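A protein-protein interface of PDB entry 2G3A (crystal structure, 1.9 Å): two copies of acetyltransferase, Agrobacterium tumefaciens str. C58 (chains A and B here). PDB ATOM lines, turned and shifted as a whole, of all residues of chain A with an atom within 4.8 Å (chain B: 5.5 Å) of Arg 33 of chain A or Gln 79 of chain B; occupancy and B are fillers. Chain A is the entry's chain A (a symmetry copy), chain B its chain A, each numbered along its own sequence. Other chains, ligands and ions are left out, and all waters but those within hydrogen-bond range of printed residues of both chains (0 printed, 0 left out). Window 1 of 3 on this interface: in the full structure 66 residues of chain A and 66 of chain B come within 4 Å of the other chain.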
ATOM      1  N   GLU A  29       5.892   4.889 -25.397  1.00  0.00           N
ATOM      2  CA  GLU A  29       4.664   5.677 -25.323  1.00  0.00           C
ATOM      3  C   GLU A  29       4.379   6.435 -26.617  1.00  0.00           C
ATOM      4  O   GLU A  29       3.221   6.555 -27.014  1.00  0.00           O
ATOM      5  CB  GLU A  29       4.711   6.646 -24.150  1.00  0.00           C
ATOM      6  CG  GLU A  29       4.416   5.994 -22.815  1.00  0.00           C
ATOM      7  CD  GLU A  29       4.429   6.988 -21.674  1.00  0.00           C
ATOM      8  OE1 GLU A  29       3.646   7.966 -21.719  1.00  0.00           O
ATOM      9  OE2 GLU A  29       5.227   6.785 -20.734  1.00  0.00           O
ATOM     10  N   LYS A  30       5.437   6.946 -27.255  1.00  0.00           N
ATOM     11  CA  LYS A  30       5.334   7.601 -28.566  1.00  0.00           C
ATOM     12  C   LYS A  30       4.856   6.611 -29.641  1.00  0.00           C
ATOM     13  O   LYS A  30       4.010   6.947 -30.476  1.00  0.00           O
ATOM     14  CB  LYS A  30       6.677   8.236 -28.966  1.00  0.00           C
ATOM     15  CG  LYS A  30       6.622   9.072 -30.233  1.00  0.00           C
ATOM     16  CD  LYS A  30       7.927   9.819 -30.479  1.00  0.00           C
ATOM     17  CE  LYS A  30       7.812  10.784 -31.656  1.00  0.00           C
ATOM     18  NZ  LYS A  30       7.738  10.071 -32.966  1.00  0.00           N
ATOM     19  N   ALA A  31       5.383   5.386 -29.587  1.00  0.00           N
ATOM     20  CA  ALA A  31       5.071   4.344 -30.567  1.00  0.00           C
ATOM     21  C   ALA A  31       3.617   3.878 -30.492  1.00  0.00           C
ATOM     22  O   ALA A  31       3.126   3.232 -31.417  1.00  0.00           O
ATOM     23  CB  ALA A  31       6.011   3.159 -30.398  1.00  0.00           C
ATOM     24  N   ILE A  32       2.948   4.201 -29.389  1.00  0.00           N
ATOM     25  CA  ILE A  32       1.510   3.937 -29.219  1.00  0.00           C
ATOM     26  C   ILE A  32       0.691   5.198 -29.533  1.00  0.00           C
ATOM     27  O   ILE A  32      -0.328   5.124 -30.216  1.00  0.00           O
ATOM     28  CB  ILE A  32       1.195   3.434 -27.783  1.00  0.00           C
ATOM     29  CG1 ILE A  32       1.856   2.073 -27.535  1.00  0.00           C
ATOM     30  CG2 ILE A  32      -0.320   3.338 -27.552  1.00  0.00           C
ATOM     31  CD1 ILE A  32       1.817   1.623 -26.080  1.00  0.00           C
ATOM     32  N   ARG A  33       1.159   6.354 -29.055  1.00  0.00           N
ATOM     33  CA  ARG A  33       0.463   7.620 -29.301  1.00  0.00           C
ATOM     34  C   ARG A  33       0.413   8.018 -30.783  1.00  0.00           C
ATOM     35  O   ARG A  33      -0.635   8.408 -31.285  1.00  0.00           O
ATOM     36  CB  ARG A  33       1.056   8.765 -28.465  1.00  0.00           C
ATOM     37  CG  ARG A  33       0.149   9.997 -28.427  1.00  0.00           C
ATOM     38  CD  ARG A  33       0.795  11.192 -27.759  1.00  0.00           C
ATOM     39  NE  ARG A  33       1.277  10.889 -26.410  1.00  0.00           N
ATOM     40  CZ  ARG A  33       0.553  11.016 -25.301  1.00  0.00           C
ATOM     41  NH1 ARG A  33      -0.709  11.442 -25.355  1.00  0.00           N
ATOM     42  NH2 ARG A  33       1.097  10.712 -24.130  1.00  0.00           N
ATOM     43  N   ASP A  34       1.538   7.933 -31.480  1.00  0.00           N
ATOM     44  CA  ASP A  34       1.582   8.421 -32.866  1.00  0.00           C
ATOM     45  C   ASP A  34       0.545   7.756 -33.795  1.00  0.00           C
ATOM     46  O   ASP A  34      -0.246   8.463 -34.427  1.00  0.00           O
ATOM     47  CB  ASP A  34       3.008   8.394 -33.431  1.00  0.00           C
ATOM     48  CG  ASP A  34       3.869   9.505 -32.866  1.00  0.00           C
ATOM     49  OD1 ASP A  34       3.343  10.316 -32.067  1.00  0.00           O
ATOM     50  OD2 ASP A  34       5.068   9.564 -33.201  1.00  0.00           O
ATOM     51  N   PRO A  35       0.512   6.404 -33.857  1.00  0.00           N
ATOM     52  CA  PRO A  35      -0.500   5.801 -34.728  1.00  0.00           C
ATOM     53  C   PRO A  35      -1.955   6.045 -34.292  1.00  0.00           C
ATOM     54  O   PRO A  35      -2.845   6.075 -35.141  1.00  0.00           O
ATOM     55  CB  PRO A  35      -0.155   4.306 -34.696  1.00  0.00           C
ATOM     56  CG  PRO A  35       0.566   4.114 -33.425  1.00  0.00           C
ATOM     57  CD  PRO A  35       1.358   5.378 -33.221  1.00  0.00           C
ATOM     58  N   LEU A  36      -2.190   6.235 -32.995  1.00  0.00           N
ATOM     59  CA  LEU A  36      -3.533   6.535 -32.505  1.00  0.00           C
ATOM     60  C   LEU A  36      -3.934   7.945 -32.948  1.00  0.00           C
ATOM     61  O   LEU A  36      -5.065   8.169 -33.369  1.00  0.00           O
ATOM     62  CB  LEU A  36      -3.600   6.404 -30.981  1.00  0.00           C
ATOM     63  CG  LEU A  36      -4.898   6.816 -30.277  1.00  0.00           C
ATOM     64  CD1 LEU A  36      -6.104   5.990 -30.768  1.00  0.00           C
ATOM     65  CD2 LEU A  36      -4.729   6.695 -28.777  1.00  0.00           C
ATOM     66  N   VAL A  37      -2.998   8.885 -32.854  1.00  0.00           N
ATOM     67  CA  VAL A  37      -3.204  10.240 -33.389  1.00  0.00           C
ATOM     68  C   VAL A  37      -3.464  10.192 -34.905  1.00  0.00           C
ATOM     69  O   VAL A  37      -4.386  10.840 -35.398  1.00  0.00           O
ATOM     70  CB  VAL A  37      -2.042  11.218 -33.004  1.00  0.00           C
ATOM     71  CG1 VAL A  37      -2.252  12.603 -33.617  1.00  0.00           C
ATOM     72  CG2 VAL A  37      -1.927  11.340 -31.491  1.00  0.00           C
ATOM     73  N   VAL B  68      -1.384   2.640 -22.591  1.00  0.00           N
ATOM     74  CA  VAL B  68      -0.617   3.538 -21.720  1.00  0.00           C
ATOM     75  C   VAL B  68      -1.539   4.038 -20.622  1.00  0.00           C
ATOM     76  O   VAL B  68      -2.626   4.564 -20.899  1.00  0.00           O
ATOM     77  CB  VAL B  68      -0.026   4.736 -22.510  1.00  0.00           C
ATOM     78  CG1 VAL B  68       0.746   5.702 -21.574  1.00  0.00           C
ATOM     79  CG2 VAL B  68       0.896   4.244 -23.621  1.00  0.00           C
ATOM     80  N   GLY B  69      -1.132   3.857 -19.374  1.00  0.00           N
ATOM     81  CA  GLY B  69      -1.919   4.386 -18.266  1.00  0.00           C
ATOM     82  C   GLY B  69      -1.142   4.491 -16.984  1.00  0.00           C
ATOM     83  O   GLY B  69       0.084   4.486 -16.988  1.00  0.00           O
ATOM     84  N   TYR B  77      -6.154   4.671 -14.425  1.00  0.00           N
ATOM     85  CA  TYR B  77      -6.560   5.520 -15.553  1.00  0.00           C
ATOM     86  C   TYR B  77      -5.891   4.956 -16.798  1.00  0.00           C
ATOM     87  O   TYR B  77      -4.659   4.796 -16.835  1.00  0.00           O
ATOM     88  CB  TYR B  77      -6.163   6.998 -15.365  1.00  0.00           C
ATOM     89  CG  TYR B  77      -6.537   7.855 -16.588  1.00  0.00           C
ATOM     90  CD1 TYR B  77      -7.835   7.849 -17.078  1.00  0.00           C
ATOM     91  CD2 TYR B  77      -5.570   8.618 -17.283  1.00  0.00           C
ATOM     92  CE1 TYR B  77      -8.198   8.603 -18.210  1.00  0.00           C
ATOM     93  CE2 TYR B  77      -5.928   9.379 -18.435  1.00  0.00           C
ATOM     94  CZ  TYR B  77      -7.248   9.357 -18.884  1.00  0.00           C
ATOM     95  OH  TYR B  77      -7.655  10.091 -20.000  1.00  0.00           O
ATOM     96  N   VAL B  78      -6.704   4.629 -17.798  1.00  0.00           N
ATOM     97  CA  VAL B  78      -6.196   4.222 -19.101  1.00  0.00           C
ATOM     98  C   VAL B  78      -6.159   5.474 -19.971  1.00  0.00           C
ATOM     99  O   VAL B  78      -7.203   6.064 -20.270  1.00  0.00           O
ATOM    100  CB  VAL B  78      -7.064   3.111 -19.752  1.00  0.00           C
ATOM    101  CG1 VAL B  78      -6.610   2.821 -21.198  1.00  0.00           C
ATOM    102  CG2 VAL B  78      -7.037   1.834 -18.903  1.00  0.00           C
ATOM    103  N   GLN B  79      -4.950   5.886 -20.354  1.00  0.00           N
ATOM    104  CA  GLN B  79      -4.759   7.109 -21.134  1.00  0.00           C
ATOM    105  C   GLN B  79      -4.809   6.885 -22.652  1.00  0.00           C
ATOM    106  O   GLN B  79      -5.451   7.656 -23.388  1.00  0.00           O
ATOM    107  CB  GLN B  79      -3.416   7.761 -20.767  1.00  0.00           C
ATOM    108  CG  GLN B  79      -3.177   9.112 -21.435  1.00  0.00           C
ATOM    109  CD  GLN B  79      -1.697   9.465 -21.518  1.00  0.00           C
ATOM    110  OE1 GLN B  79      -0.871   8.936 -20.763  1.00  0.00           O
ATOM    111  NE2 GLN B  79      -1.355  10.359 -22.440  1.00  0.00           N
ATOM    112  N   LEU B  80      -4.121   5.847 -23.127  1.00  0.00           N
ATOM    113  CA  LEU B  80      -4.085   5.561 -24.554  1.00  0.00           C
ATOM    114  C   LEU B  80      -4.260   4.080 -24.760  1.00  0.00           C
ATOM    115  O   LEU B  80      -3.746   3.290 -23.982  1.00  0.00           O
ATOM    116  CB  LEU B  80      -2.743   5.970 -25.181  1.00  0.00           C
ATOM    117  CG  LEU B  80      -2.136   7.366 -24.978  1.00  0.00           C
ATOM    118  CD1 LEU B  80      -0.672   7.339 -25.401  1.00  0.00           C
ATOM    119  CD2 LEU B  80      -2.883   8.420 -25.769  1.00  0.00           C
ATOM    120  N   LEU B  81      -4.956   3.716 -25.834  1.00  0.00           N
ATOM    121  CA  LEU B  81      -5.060   2.329 -26.252  1.00  0.00           C
ATOM    122  C   LEU B  81      -5.116   2.298 -27.752  1.00  0.00           C
ATOM    123  O   LEU B  81      -6.002   2.919 -28.352  1.00  0.00           O
ATOM    124  CB  LEU B  81      -6.318   1.678 -25.671  1.00  0.00           C
ATOM    125  CG  LEU B  81      -6.435   0.150 -25.666  1.00  0.00           C
ATOM    126  CD1 LEU B  81      -7.454  -0.301 -24.633  1.00  0.00           C
ATOM    127  CD2 LEU B  81      -6.783  -0.438 -27.049  1.00  0.00           C
ATOM    128  N   ASP B 115     -11.703   7.366 -20.955  1.00  0.00           N
ATOM    129  CA  ASP B 115     -12.520   8.311 -21.724  1.00  0.00           C
ATOM    130  C   ASP B 115     -12.307   8.136 -23.222  1.00  0.00           C
ATOM    131  O   ASP B 115     -11.313   7.563 -23.643  1.00  0.00           O
ATOM    132  CB  ASP B 115     -12.241   9.743 -21.283  1.00  0.00           C
ATOM    133  CG  ASP B 115     -10.770  10.056 -21.279  1.00  0.00           C
ATOM    134  OD1 ASP B 115     -10.201  10.121 -22.369  1.00  0.00           O
ATOM    135  OD2 ASP B 115     -10.194  10.211 -20.190  1.00  0.00           O
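NH2 of Arg 33 of chain A sits close to NE2 of Gln 79 of chain B.
O of Leu 80 of chain B is in hydrogen-bond range of N of Val 68 of chain B, at 2.8 Å. The backbone carbonyl oxygen of Val 68 of chain B is in hydrogen-bond range of the backbone NH of Gln 79 of chain B (2.7 Å).
Among the printed residues, pairs that only touch across the chains: Glu 29 of chain A with Val 68 of chain B (3.7 Å), Ile 32 of chain A with Val 68 of chain B (3.7 Å), Arg 33 of chain A with Leu 80 of chain B (3.7 Å), Leu 36 of chain A with Leu 81 of chain B (3.9 Å) and Leu 36 of chain A with Leu 80 of chain B (3.9 Å).
Of the printed residues of chain B, Glu 29 of chain A touches Val 68. Arg 33 of chain A touches just these residues of chain B: Gln 79 and Leu 80. Of the printed residues of chain B, Leu 36 of chain A touches Leu 80 (3.9 Å) and Leu 81 (3.9 Å). Of the printed residues of chain A, Val 68 of chain B touches Glu 29 (3.7 Å) and Ile 32 (3.7 Å). Val 78 of chain B touches none of the printed residues of chain A. Gln 79 of chain B touches one residue of chain A. Printed residues of chain A within 4 Å of Leu 80 of chain B: Arg 33 (3.7 Å) and Leu 36 (3.9 Å). Printed residues of chain A within 4 Å of Leu 81 of chain B: Leu 36.
Of the 8 printed residues of chain B, 4 touch a printed residue of chain A. Hydrophobic or aromatic side chains of chain B that line the printed part of chain A: Val 68 and Leu 80. Printed residues of chain A that touch a printed residue of chain B: Glu 29, Ile 32, Arg 33 and Leu 36. Hydrophobic or aromatic side chains of chain A within 4 Å of the printed part of chain B: Ile 32 and Leu 36. Along chain A the printed residues that touch a printed residue of chain B span positions 29 to 36. Among the printed residues, no Asp or Glu carboxylate lies within 4 Å of a Lys or Arg side-chain nitrogen of the other chain.
No position is printed for both chains. Of the 6 pairs that touch across the chains among the printed residues, none has its exchanged pair printed and touching as well.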
